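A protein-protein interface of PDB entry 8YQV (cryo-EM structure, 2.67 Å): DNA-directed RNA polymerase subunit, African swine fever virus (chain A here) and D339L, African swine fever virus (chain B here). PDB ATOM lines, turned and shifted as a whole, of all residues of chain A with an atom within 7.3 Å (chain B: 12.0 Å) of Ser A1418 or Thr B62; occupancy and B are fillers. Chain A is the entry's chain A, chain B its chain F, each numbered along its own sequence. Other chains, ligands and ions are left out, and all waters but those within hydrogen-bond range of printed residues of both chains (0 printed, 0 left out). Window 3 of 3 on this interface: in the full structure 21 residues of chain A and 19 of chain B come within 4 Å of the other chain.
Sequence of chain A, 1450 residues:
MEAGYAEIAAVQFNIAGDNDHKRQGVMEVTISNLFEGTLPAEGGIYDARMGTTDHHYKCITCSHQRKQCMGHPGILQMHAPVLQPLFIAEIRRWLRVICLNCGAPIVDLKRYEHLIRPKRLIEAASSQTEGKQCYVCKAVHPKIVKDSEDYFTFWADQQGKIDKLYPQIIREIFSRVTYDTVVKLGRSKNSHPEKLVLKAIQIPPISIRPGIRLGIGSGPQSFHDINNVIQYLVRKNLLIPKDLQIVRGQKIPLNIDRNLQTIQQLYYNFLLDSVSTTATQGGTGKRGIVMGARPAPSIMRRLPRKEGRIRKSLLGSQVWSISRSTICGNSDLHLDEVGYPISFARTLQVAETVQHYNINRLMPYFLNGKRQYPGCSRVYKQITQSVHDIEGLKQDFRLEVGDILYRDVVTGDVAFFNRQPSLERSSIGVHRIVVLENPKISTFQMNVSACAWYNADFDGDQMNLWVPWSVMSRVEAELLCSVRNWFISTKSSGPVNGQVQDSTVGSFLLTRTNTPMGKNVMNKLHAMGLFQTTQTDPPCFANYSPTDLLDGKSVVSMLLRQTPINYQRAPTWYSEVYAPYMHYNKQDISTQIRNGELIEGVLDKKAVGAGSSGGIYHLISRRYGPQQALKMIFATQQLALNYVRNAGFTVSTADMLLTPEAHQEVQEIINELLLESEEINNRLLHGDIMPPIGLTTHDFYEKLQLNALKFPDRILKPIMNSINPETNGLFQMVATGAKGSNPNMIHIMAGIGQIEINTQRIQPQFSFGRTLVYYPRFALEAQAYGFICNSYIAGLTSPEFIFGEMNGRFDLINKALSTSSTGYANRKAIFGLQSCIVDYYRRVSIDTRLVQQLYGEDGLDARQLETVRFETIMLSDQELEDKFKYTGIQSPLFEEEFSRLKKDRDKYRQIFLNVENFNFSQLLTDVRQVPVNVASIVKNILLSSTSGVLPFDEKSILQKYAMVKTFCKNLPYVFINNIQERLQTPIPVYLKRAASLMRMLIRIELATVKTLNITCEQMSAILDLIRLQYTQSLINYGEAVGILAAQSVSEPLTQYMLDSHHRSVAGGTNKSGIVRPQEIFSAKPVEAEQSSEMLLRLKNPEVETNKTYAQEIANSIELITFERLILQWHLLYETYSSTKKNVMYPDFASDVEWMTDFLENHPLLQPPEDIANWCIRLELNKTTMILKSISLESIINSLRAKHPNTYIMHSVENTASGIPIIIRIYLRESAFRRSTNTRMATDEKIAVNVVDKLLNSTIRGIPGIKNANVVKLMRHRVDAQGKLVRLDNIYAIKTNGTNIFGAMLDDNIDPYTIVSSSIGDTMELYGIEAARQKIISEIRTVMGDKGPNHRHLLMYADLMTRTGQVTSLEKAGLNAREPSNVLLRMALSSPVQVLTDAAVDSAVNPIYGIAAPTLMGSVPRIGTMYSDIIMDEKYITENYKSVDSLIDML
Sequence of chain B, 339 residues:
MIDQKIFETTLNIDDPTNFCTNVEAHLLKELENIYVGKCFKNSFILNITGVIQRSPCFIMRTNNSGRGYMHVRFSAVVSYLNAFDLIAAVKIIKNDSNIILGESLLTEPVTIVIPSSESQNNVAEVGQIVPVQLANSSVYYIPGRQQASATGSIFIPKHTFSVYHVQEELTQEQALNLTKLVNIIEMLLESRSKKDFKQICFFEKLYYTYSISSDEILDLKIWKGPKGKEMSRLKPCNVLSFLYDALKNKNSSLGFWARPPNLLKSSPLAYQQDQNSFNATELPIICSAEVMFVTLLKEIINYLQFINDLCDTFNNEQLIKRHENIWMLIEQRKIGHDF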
ATOM      1  N   TYR A   5      25.273 -24.074   0.223  1.00  0.00           N
ATOM      2  CA  TYR A   5      24.162 -24.634  -0.530  1.00  0.00           C
ATOM      3  C   TYR A   5      24.597 -24.991  -1.944  1.00  0.00           C
ATOM      4  O   TYR A   5      25.220 -24.181  -2.635  1.00  0.00           O
ATOM      5  CB  TYR A   5      23.012 -23.631  -0.571  1.00  0.00           C
ATOM      6  CG  TYR A   5      21.851 -24.039  -1.440  1.00  0.00           C
ATOM      7  CD1 TYR A   5      20.863 -24.870  -0.962  1.00  0.00           C
ATOM      8  CD2 TYR A   5      21.746 -23.587  -2.739  1.00  0.00           C
ATOM      9  CE1 TYR A   5      19.807 -25.235  -1.753  1.00  0.00           C
ATOM     10  CE2 TYR A   5      20.699 -23.948  -3.533  1.00  0.00           C
ATOM     11  CZ  TYR A   5      19.733 -24.770  -3.039  1.00  0.00           C
ATOM     12  OH  TYR A   5      18.683 -25.130  -3.842  1.00  0.00           O
ATOM     13  N   ALA A   6      24.245 -26.195  -2.386  1.00  0.00           N
ATOM     14  CA  ALA A   6      24.610 -26.658  -3.713  1.00  0.00           C
ATOM     15  C   ALA A   6      23.430 -27.376  -4.345  1.00  0.00           C
ATOM     16  O   ALA A   6      22.465 -27.745  -3.675  1.00  0.00           O
ATOM     17  CB  ALA A   6      25.827 -27.583  -3.674  1.00  0.00           C
ATOM     18  N   GLU A   7      23.511 -27.550  -5.657  1.00  0.00           N
ATOM     19  CA  GLU A   7      22.551 -28.336  -6.413  1.00  0.00           C
ATOM     20  C   GLU A   7      23.308 -29.222  -7.384  1.00  0.00           C
ATOM     21  O   GLU A   7      24.324 -28.809  -7.943  1.00  0.00           O
ATOM     22  CB  GLU A   7      21.570 -27.442  -7.170  1.00  0.00           C
ATOM     23  CG  GLU A   7      20.611 -26.694  -6.270  1.00  0.00           C
ATOM     24  CD  GLU A   7      19.824 -25.626  -6.993  1.00  0.00           C
ATOM     25  OE1 GLU A   7      20.058 -25.421  -8.199  1.00  0.00           O
ATOM     26  OE2 GLU A   7      18.979 -24.977  -6.347  1.00  0.00           O
ATOM     27  N   ILE A   8      22.814 -30.437  -7.583  1.00  0.00           N
ATOM     28  CA  ILE A   8      23.440 -31.362  -8.518  1.00  0.00           C
ATOM     29  C   ILE A   8      23.071 -30.943  -9.934  1.00  0.00           C
ATOM     30  O   ILE A   8      21.891 -30.787 -10.260  1.00  0.00           O
ATOM     31  CB  ILE A   8      23.016 -32.808  -8.237  1.00  0.00           C
ATOM     32  CG1 ILE A   8      23.570 -33.268  -6.891  1.00  0.00           C
ATOM     33  CG2 ILE A   8      23.484 -33.725  -9.341  1.00  0.00           C
ATOM     34  CD1 ILE A   8      23.031 -34.589  -6.438  1.00  0.00           C
ATOM     35  N   ILE A1407      21.083 -32.943 -15.372  1.00  0.00           N
ATOM     36  CA  ILE A1407      19.842 -32.978 -14.612  1.00  0.00           C
ATOM     37  C   ILE A1407      18.886 -31.959 -15.220  1.00  0.00           C
ATOM     38  O   ILE A1407      19.146 -30.755 -15.197  1.00  0.00           O
ATOM     39  CB  ILE A1407      20.085 -32.708 -13.123  1.00  0.00           C
ATOM     40  CG1 ILE A1407      20.968 -33.801 -12.520  1.00  0.00           C
ATOM     41  CG2 ILE A1407      18.782 -32.649 -12.374  1.00  0.00           C
ATOM     42  CD1 ILE A1407      20.396 -35.185 -12.630  1.00  0.00           C
ATOM     43  N   ILE A1410      11.770 -33.830 -15.355  1.00  0.00           N
ATOM     44  CA  ILE A1410      11.091 -34.197 -14.119  1.00  0.00           C
ATOM     45  C   ILE A1410      11.760 -35.390 -13.451  1.00  0.00           C
ATOM     46  O   ILE A1410      12.114 -35.334 -12.277  1.00  0.00           O
ATOM     47  CB  ILE A1410       9.590 -34.479 -14.364  1.00  0.00           C
ATOM     48  CG1 ILE A1410       8.809 -33.192 -14.577  1.00  0.00           C
ATOM     49  CG2 ILE A1410       8.989 -35.220 -13.196  1.00  0.00           C
ATOM     50  CD1 ILE A1410       8.769 -32.747 -15.983  1.00  0.00           C
ATOM     51  N   ALA A1412      14.696 -37.046 -13.908  1.00  0.00           N
ATOM     52  CA  ALA A1412      16.093 -36.991 -13.498  1.00  0.00           C
ATOM     53  C   ALA A1412      16.254 -36.282 -12.155  1.00  0.00           C
ATOM     54  O   ALA A1412      16.925 -36.822 -11.271  1.00  0.00           O
ATOM     55  CB  ALA A1412      16.953 -36.328 -14.576  1.00  0.00           C
ATOM     56  N   PRO A1413      15.679 -35.088 -11.941  1.00  0.00           N
ATOM     57  CA  PRO A1413      15.767 -34.479 -10.607  1.00  0.00           C
ATOM     58  C   PRO A1413      15.015 -35.235  -9.533  1.00  0.00           C
ATOM     59  O   PRO A1413      15.409 -35.166  -8.366  1.00  0.00           O
ATOM     60  CB  PRO A1413      15.168 -33.084 -10.814  1.00  0.00           C
ATOM     61  CG  PRO A1413      15.242 -32.847 -12.237  1.00  0.00           C
ATOM     62  CD  PRO A1413      15.040 -34.157 -12.884  1.00  0.00           C
ATOM     63  N   THR A1414      13.937 -35.935  -9.873  1.00  0.00           N
ATOM     64  CA  THR A1414      13.165 -36.645  -8.862  1.00  0.00           C
ATOM     65  C   THR A1414      13.922 -37.854  -8.329  1.00  0.00           C
ATOM     66  O   THR A1414      13.870 -38.145  -7.129  1.00  0.00           O
ATOM     67  CB  THR A1414      11.818 -37.060  -9.446  1.00  0.00           C
ATOM     68  OG1 THR A1414      11.097 -35.890  -9.841  1.00  0.00           O
ATOM     69  CG2 THR A1414      11.000 -37.827  -8.435  1.00  0.00           C
ATOM     70  N   LEU A1415      14.632 -38.571  -9.201  1.00  0.00           N
ATOM     71  CA  LEU A1415      15.400 -39.729  -8.761  1.00  0.00           C
ATOM     72  C   LEU A1415      16.626 -39.320  -7.958  1.00  0.00           C
ATOM     73  O   LEU A1415      17.106 -40.095  -7.127  1.00  0.00           O
ATOM     74  CB  LEU A1415      15.806 -40.574  -9.965  1.00  0.00           C
ATOM     75  CG  LEU A1415      14.900 -41.758 -10.302  1.00  0.00           C
ATOM     76  CD1 LEU A1415      13.508 -41.295 -10.640  1.00  0.00           C
ATOM     77  CD2 LEU A1415      15.470 -42.553 -11.449  1.00  0.00           C
ATOM     78  N   MET A1416      17.134 -38.116  -8.177  1.00  0.00           N
ATOM     79  CA  MET A1416      18.265 -37.594  -7.427  1.00  0.00           C
ATOM     80  C   MET A1416      17.845 -36.904  -6.139  1.00  0.00           C
ATOM     81  O   MET A1416      18.690 -36.299  -5.473  1.00  0.00           O
ATOM     82  CB  MET A1416      19.067 -36.629  -8.296  1.00  0.00           C
ATOM     83  CG  MET A1416      19.992 -37.318  -9.267  1.00  0.00           C
ATOM     84  SD  MET A1416      21.311 -38.216  -8.443  1.00  0.00           S
ATOM     85  CE  MET A1416      21.019 -39.859  -9.070  1.00  0.00           C
ATOM     86  N   GLY A1417      16.566 -36.966  -5.784  1.00  0.00           N
ATOM     87  CA  GLY A1417      16.074 -36.387  -4.556  1.00  0.00           C
ATOM     88  C   GLY A1417      15.802 -34.905  -4.605  1.00  0.00           C
ATOM     89  O   GLY A1417      15.430 -34.331  -3.578  1.00  0.00           O
ATOM     90  N   SER A1418      15.969 -34.269  -5.755  1.00  0.00           N
ATOM     91  CA  SER A1418      15.755 -32.839  -5.891  1.00  0.00           C
ATOM     92  C   SER A1418      14.367 -32.584  -6.476  1.00  0.00           C
ATOM     93  O   SER A1418      13.558 -33.499  -6.635  1.00  0.00           O
ATOM     94  CB  SER A1418      16.861 -32.231  -6.742  1.00  0.00           C
ATOM     95  OG  SER A1418      16.691 -30.834  -6.854  1.00  0.00           O
ATOM     96  N   VAL A1419      14.074 -31.329  -6.801  1.00  0.00           N
ATOM     97  CA  VAL A1419      12.791 -30.973  -7.399  1.00  0.00           C
ATOM     98  C   VAL A1419      13.028 -30.446  -8.809  1.00  0.00           C
ATOM     99  O   VAL A1419      14.063 -29.818  -9.070  1.00  0.00           O
ATOM    100  CB  VAL A1419      12.036 -29.947  -6.540  1.00  0.00           C
ATOM    101  CG1 VAL A1419      11.659 -30.555  -5.214  1.00  0.00           C
ATOM    102  CG2 VAL A1419      12.876 -28.710  -6.328  1.00  0.00           C
ATOM    103  N   PRO A1420      12.114 -30.690  -9.744  1.00  0.00           N
ATOM    104  CA  PRO A1420      12.284 -30.162 -11.100  1.00  0.00           C
ATOM    105  C   PRO A1420      12.302 -28.641 -11.135  1.00  0.00           C
ATOM    106  O   PRO A1420      11.585 -27.971 -10.394  1.00  0.00           O
ATOM    107  CB  PRO A1420      11.069 -30.719 -11.845  1.00  0.00           C
ATOM    108  CG  PRO A1420      10.677 -31.910 -11.078  1.00  0.00           C
ATOM    109  CD  PRO A1420      10.968 -31.604  -9.653  1.00  0.00           C
ATOM    110  N   ARG A1421      13.134 -28.099 -12.020  1.00  0.00           N
ATOM    111  CA  ARG A1421      13.175 -26.662 -12.275  1.00  0.00           C
ATOM    112  C   ARG A1421      12.054 -26.341 -13.257  1.00  0.00           C
ATOM    113  O   ARG A1421      12.231 -26.296 -14.473  1.00  0.00           O
ATOM    114  CB  ARG A1421      14.542 -26.252 -12.799  1.00  0.00           C
ATOM    115  CG  ARG A1421      14.646 -24.809 -13.217  1.00  0.00           C
ATOM    116  CD  ARG A1421      16.081 -24.368 -13.266  1.00  0.00           C
ATOM    117  NE  ARG A1421      16.864 -24.999 -12.212  1.00  0.00           N
ATOM    118  CZ  ARG A1421      18.102 -24.650 -11.892  1.00  0.00           C
ATOM    119  NH1 ARG A1421      18.737 -23.691 -12.542  1.00  0.00           N
ATOM    120  NH2 ARG A1421      18.716 -25.280 -10.897  1.00  0.00           N
ATOM    121  N   MET A1425       9.615 -22.782  -9.857  1.00  0.00           N
ATOM    122  CA  MET A1425      11.059 -22.844  -9.716  1.00  0.00           C
ATOM    123  C   MET A1425      11.789 -22.660 -11.027  1.00  0.00           C
ATOM    124  O   MET A1425      12.992 -22.910 -11.088  1.00  0.00           O
ATOM    125  CB  MET A1425      11.463 -24.166  -9.088  1.00  0.00           C
ATOM    126  CG  MET A1425      10.604 -24.482  -7.928  1.00  0.00           C
ATOM    127  SD  MET A1425      11.204 -23.752  -6.421  1.00  0.00           S
ATOM    128  CE  MET A1425      10.734 -25.057  -5.331  1.00  0.00           C
ATOM    129  N   THR B  10      30.718 -20.904  -0.679  1.00  0.00           N
ATOM    130  CA  THR B  10      29.312 -20.529  -0.751  1.00  0.00           C
ATOM    131  C   THR B  10      28.805 -20.340   0.668  1.00  0.00           C
ATOM    132  O   THR B  10      28.852 -21.274   1.474  1.00  0.00           O
ATOM    133  CB  THR B  10      28.477 -21.579  -1.482  1.00  0.00           C
ATOM    134  OG1 THR B  10      28.941 -21.714  -2.826  1.00  0.00           O
ATOM    135  CG2 THR B  10      27.029 -21.164  -1.514  1.00  0.00           C
ATOM    136  N   ASN B  12      25.755 -19.577   3.339  1.00  0.00           N
ATOM    137  CA  ASN B  12      24.321 -19.620   3.583  1.00  0.00           C
ATOM    138  C   ASN B  12      23.912 -18.415   4.415  1.00  0.00           C
ATOM    139  O   ASN B  12      24.539 -18.114   5.435  1.00  0.00           O
ATOM    140  CB  ASN B  12      23.934 -20.905   4.305  1.00  0.00           C
ATOM    141  CG  ASN B  12      24.293 -22.132   3.526  1.00  0.00           C
ATOM    142  OD1 ASN B  12      24.187 -22.154   2.306  1.00  0.00           O
ATOM    143  ND2 ASN B  12      24.725 -23.167   4.221  1.00  0.00           N
ATOM    144  N   PHE B  58      21.198 -15.282  -3.985  1.00  0.00           N
ATOM    145  CA  PHE B  58      20.169 -16.158  -4.513  1.00  0.00           C
ATOM    146  C   PHE B  58      19.336 -16.738  -3.384  1.00  0.00           C
ATOM    147  O   PHE B  58      19.834 -16.995  -2.289  1.00  0.00           O
ATOM    148  CB  PHE B  58      20.783 -17.301  -5.314  1.00  0.00           C
ATOM    149  CG  PHE B  58      21.698 -16.860  -6.408  1.00  0.00           C
ATOM    150  CD1 PHE B  58      21.192 -16.329  -7.575  1.00  0.00           C
ATOM    151  CD2 PHE B  58      23.063 -17.000  -6.282  1.00  0.00           C
ATOM    152  CE1 PHE B  58      22.028 -15.930  -8.584  1.00  0.00           C
ATOM    153  CE2 PHE B  58      23.902 -16.605  -7.293  1.00  0.00           C
ATOM    154  CZ  PHE B  58      23.382 -16.068  -8.445  1.00  0.00           C
ATOM    155  N   ILE B  59      18.073 -16.960  -3.661  1.00  0.00           N
ATOM    156  CA  ILE B  59      17.175 -17.615  -2.722  1.00  0.00           C
ATOM    157  C   ILE B  59      17.223 -19.109  -2.980  1.00  0.00           C
ATOM    158  O   ILE B  59      17.097 -19.553  -4.123  1.00  0.00           O
ATOM    159  CB  ILE B  59      15.745 -17.065  -2.859  1.00  0.00           C
ATOM    160  CG1 ILE B  59      15.755 -15.544  -2.780  1.00  0.00           C
ATOM    161  CG2 ILE B  59      14.854 -17.632  -1.789  1.00  0.00           C
ATOM    162  CD1 ILE B  59      16.351 -15.014  -1.523  1.00  0.00           C
ATOM    163  N   MET B  60      17.426 -19.890  -1.922  1.00  0.00           N
ATOM    164  CA  MET B  60      17.570 -21.330  -2.079  1.00  0.00           C
ATOM    165  C   MET B  60      16.297 -21.936  -2.646  1.00  0.00           C
ATOM    166  O   MET B  60      15.188 -21.616  -2.217  1.00  0.00           O
ATOM    167  CB  MET B  60      17.939 -21.981  -0.748  1.00  0.00           C
ATOM    168  CG  MET B  60      19.095 -21.282  -0.058  1.00  0.00           C
ATOM    169  SD  MET B  60      19.689 -22.034   1.465  1.00  0.00           S
ATOM    170  CE  MET B  60      18.383 -23.195   1.770  1.00  0.00           C
ATOM    171  N   ARG B  61      16.471 -22.819  -3.622  1.00  0.00           N
ATOM    172  CA  ARG B  61      15.388 -23.259  -4.484  1.00  0.00           C
ATOM    173  C   ARG B  61      14.852 -24.637  -4.136  1.00  0.00           C
ATOM    174  O   ARG B  61      13.705 -24.933  -4.466  1.00  0.00           O
ATOM    175  CB  ARG B  61      15.872 -23.260  -5.936  1.00  0.00           C
ATOM    176  CG  ARG B  61      14.807 -23.428  -6.973  1.00  0.00           C
ATOM    177  CD  ARG B  61      15.376 -24.062  -8.223  1.00  0.00           C
ATOM    178  NE  ARG B  61      14.889 -25.422  -8.409  1.00  0.00           N
ATOM    179  CZ  ARG B  61      15.663 -26.491  -8.519  1.00  0.00           C
ATOM    180  NH1 ARG B  61      16.980 -26.397  -8.475  1.00  0.00           N
ATOM    181  NH2 ARG B  61      15.101 -27.684  -8.675  1.00  0.00           N
ATOM    182  N   THR B  62      15.637 -25.484  -3.485  1.00  0.00           N
ATOM    183  CA  THR B  62      15.251 -26.869  -3.265  1.00  0.00           C
ATOM    184  C   THR B  62      14.615 -27.103  -1.902  1.00  0.00           C
ATOM    185  O   THR B  62      14.391 -28.257  -1.529  1.00  0.00           O
ATOM    186  CB  THR B  62      16.460 -27.783  -3.448  1.00  0.00           C
ATOM    187  OG1 THR B  62      17.641 -27.091  -3.035  1.00  0.00           O
ATOM    188  CG2 THR B  62      16.609 -28.180  -4.899  1.00  0.00           C
ATOM    189  N   ASN B  63      14.326 -26.045  -1.150  1.00  0.00           N
ATOM    190  CA  ASN B  63      13.581 -26.182   0.091  1.00  0.00           C
ATOM    191  C   ASN B  63      12.791 -24.907   0.334  1.00  0.00           C
ATOM    192  O   ASN B  63      13.067 -23.860  -0.253  1.00  0.00           O
ATOM    193  CB  ASN B  63      14.491 -26.482   1.283  1.00  0.00           C
ATOM    194  CG  ASN B  63      15.582 -25.462   1.457  1.00  0.00           C
ATOM    195  OD1 ASN B  63      15.710 -24.530   0.674  1.00  0.00           O
ATOM    196  ND2 ASN B  63      16.371 -25.626   2.501  1.00  0.00           N
ATOM    197  N   ASN B  64      11.803 -25.006   1.219  1.00  0.00           N
ATOM    198  CA  ASN B  64      10.890 -23.900   1.488  1.00  0.00           C
ATOM    199  C   ASN B  64      11.358 -23.040   2.643  1.00  0.00           C
ATOM    200  O   ASN B  64      10.542 -22.476   3.370  1.00  0.00           O
ATOM    201  CB  ASN B  64       9.489 -24.436   1.758  1.00  0.00           C
ATOM    202  CG  ASN B  64       8.840 -25.027   0.533  1.00  0.00           C
ATOM    203  OD1 ASN B  64       9.132 -24.632  -0.588  1.00  0.00           O
ATOM    204  ND2 ASN B  64       7.932 -25.960   0.745  1.00  0.00           N
ATOM    205  N   SER B  65      12.665 -22.926   2.847  1.00  0.00           N
ATOM    206  CA  SER B  65      13.209 -22.199   3.982  1.00  0.00           C
ATOM    207  C   SER B  65      13.207 -20.691   3.801  1.00  0.00           C
ATOM    208  O   SER B  65      13.266 -19.966   4.798  1.00  0.00           O
ATOM    209  CB  SER B  65      14.636 -22.658   4.259  1.00  0.00           C
ATOM    210  OG  SER B  65      15.463 -22.402   3.146  1.00  0.00           O
ATOM    211  N   GLY B  66      13.137 -20.200   2.568  1.00  0.00           N
ATOM    212  CA  GLY B  66      13.207 -18.772   2.340  1.00  0.00           C
ATOM    213  C   GLY B  66      14.567 -18.177   2.580  1.00  0.00           C
ATOM    214  O   GLY B  66      14.687 -16.959   2.706  1.00  0.00           O
ATOM    215  N   ARG B  67      15.600 -19.007   2.626  1.00  0.00           N
ATOM    216  CA  ARG B  67      16.948 -18.614   2.995  1.00  0.00           C
ATOM    217  C   ARG B  67      17.753 -18.311   1.743  1.00  0.00           C
ATOM    218  O   ARG B  67      17.375 -18.685   0.632  1.00  0.00           O
ATOM    219  CB  ARG B  67      17.620 -19.721   3.803  1.00  0.00           C
ATOM    220  CG  ARG B  67      17.487 -19.557   5.295  1.00  0.00           C
ATOM    221  CD  ARG B  67      18.270 -20.619   6.027  1.00  0.00           C
ATOM    222  NE  ARG B  67      18.023 -21.947   5.483  1.00  0.00           N
ATOM    223  CZ  ARG B  67      18.903 -22.938   5.501  1.00  0.00           C
ATOM    224  NH1 ARG B  67      20.109 -22.780   6.017  1.00  0.00           N
ATOM    225  NH2 ARG B  67      18.567 -24.114   4.982  1.00  0.00           N
ATOM    226  N   GLY B  68      18.870 -17.623   1.927  1.00  0.00           N
ATOM    227  CA  GLY B  68      19.663 -17.222   0.787  1.00  0.00           C
ATOM    228  C   GLY B  68      21.008 -17.907   0.719  1.00  0.00           C
ATOM    229  O   GLY B  68      21.412 -18.577   1.666  1.00  0.00           O
ATOM    230  N   TYR B  69      21.713 -17.750  -0.393  1.00  0.00           N
ATOM    231  CA  TYR B  69      23.089 -18.205  -0.472  1.00  0.00           C
ATOM    232  C   TYR B  69      23.844 -17.292  -1.419  1.00  0.00           C
ATOM    233  O   TYR B  69      23.266 -16.684  -2.318  1.00  0.00           O
ATOM    234  CB  TYR B  69      23.186 -19.670  -0.908  1.00  0.00           C
ATOM    235  CG  TYR B  69      22.741 -19.962  -2.319  1.00  0.00           C
ATOM    236  CD1 TYR B  69      21.412 -20.218  -2.609  1.00  0.00           C
ATOM    237  CD2 TYR B  69      23.653 -20.007  -3.355  1.00  0.00           C
ATOM    238  CE1 TYR B  69      21.007 -20.497  -3.889  1.00  0.00           C
ATOM    239  CE2 TYR B  69      23.254 -20.281  -4.635  1.00  0.00           C
ATOM    240  CZ  TYR B  69      21.931 -20.528  -4.895  1.00  0.00           C
ATOM    241  OH  TYR B  69      21.534 -20.806  -6.176  1.00  0.00           O
ATOM    242  N   HIS B  71      27.768 -16.878  -3.463  1.00  0.00           N
ATOM    243  CA  HIS B  71      29.090 -17.369  -3.823  1.00  0.00           C
ATOM    244  C   HIS B  71      30.109 -16.256  -3.642  1.00  0.00           C
ATOM    245  O   HIS B  71      29.923 -15.148  -4.149  1.00  0.00           O
ATOM    246  CB  HIS B  71      29.122 -17.873  -5.263  1.00  0.00           C
ATOM    247  CG  HIS B  71      28.060 -18.876  -5.579  1.00  0.00           C
ATOM    248  ND1 HIS B  71      27.993 -20.107  -4.967  1.00  0.00           N
ATOM    249  CD2 HIS B  71      27.039 -18.842  -6.465  1.00  0.00           C
ATOM    250  CE1 HIS B  71      26.971 -20.782  -5.455  1.00  0.00           C
ATOM    251  NE2 HIS B  71      26.375 -20.037  -6.364  1.00  0.00           N
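The side-chain amide oxygen of Asn B12 lies within hydrogen-bond range of the backbone NH of Tyr A5, 3.0 Å away.
N of Arg B61 lies within hydrogen-bond range of OH of Tyr A5, 3.2 Å away.
OH of Tyr A5 is in hydrogen-bond range of N of Thr B62 (3.1 Å).
NH1 of Arg B61 lies within salt-bridge range of OE1 of Glu A7 (3.2 Å).
The backbone carbonyl oxygen (O) of Val A1419 sits at hydrogen-bond distance from the guanidinium group (NH2) of Arg B61, at 2.4 Å.
The guanidinium group (NH2) of Arg A1421 lies close to the guanidinium group (NH1) of Arg B61 (3.2 Å).
O of Arg B61 lies close to SD of Met A1425.
OH of Tyr A5 is in hydrogen-bond range of OE2 of Glu A7 (2.5 Å).
OE1 of Glu A7 lies within salt-bridge range of NH2 of Arg A1421 (3.0 Å).
The backbone carbonyl oxygen (O) of Pro A1413 is in hydrogen-bond range of the backbone NH (N) of Ser A1418 (2.8 Å).
The side-chain hydroxyl (OG1) of Thr B10 lies within hydrogen-bond range of a ring nitrogen (ND1) of His B71.
The backbone carbonyl oxygen (O) of Phe B58 is in hydrogen-bond range of the backbone NH (N) of Tyr B69 (2.8 Å).
N of Met B60 sits at hydrogen-bond distance from O of Arg B67.
O of Tyr A5 touches CG2 of Thr B10, 3.7 Å away.
CE1 of Tyr A5 touches CB of Met B60, at 3.9 Å.
Tyr A5 touches Tyr B69 (CD2 to CE1, 3.4 Å).
NH2 of Arg B61 touches OG of Ser A1418 (3.97 Å).
Thr B62 touches Ser A1418.
Pro A1420 touches Arg B61 (C to NH2, 3.8 Å).
Printed residues of chain B within 4 Å of Tyr A5: Thr B10 (3.7 Å), Asn B12 (3.0 Å), Met B60 (3.9 Å), Arg B61 (3.2 Å), Thr B62 (2.4 Å) and Tyr B69 (3.4 Å).
No residue of chain B comes within 4 Å of Ile A8.
Ala A1412 touches none of the printed residues of chain B.
No residue of chain B comes within 4 Å of Thr A1414.
No residue of chain B comes within 4 Å of Gly A1417.
Ser A1418 touches just these residues of chain B: Arg B61 and Thr B62.
Pro A1420 touches one residue of chain B.
Of the printed residues of chain B, Arg A1421 touches Arg B61 (3.2 Å).
Of the printed residues of chain B, Met A1425 touches Arg B61 (3.1 Å).
Of the printed residues of chain A, Thr B10 touches Tyr A5 (3.7 Å).
Of the printed residues of chain A, Tyr B69 touches Tyr A5.
The nearest residue of chain B that does not touch Ser A1418 is Asn B63 (7.8 Å).
The nearest printed residue of chain A that does not touch Asn B12 is Ala A6 (6.2 Å).
Of the 17 printed residues of chain A, 7 touch a printed residue of chain B.
Printed residues of chain A that touch a printed residue of chain B: Tyr A5, Glu A7, Ser A1418, Val A1419, Pro A1420, Arg A1421 and Met A1425.
Of the 15 printed residues of chain B, 6 touch a printed residue of chain A.
Hydrophobic or aromatic side chains of chain B within 4 Å of the printed part of chain A: Met B60 and Tyr B69.
Among the printed residues, 13 pairs touch across the chains.
Among the printed residues, Asp or Glu carboxylates within 4 Å of a Lys or Arg side-chain nitrogen of the other chain: Glu A7 with Arg B61 (3.2 Å).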
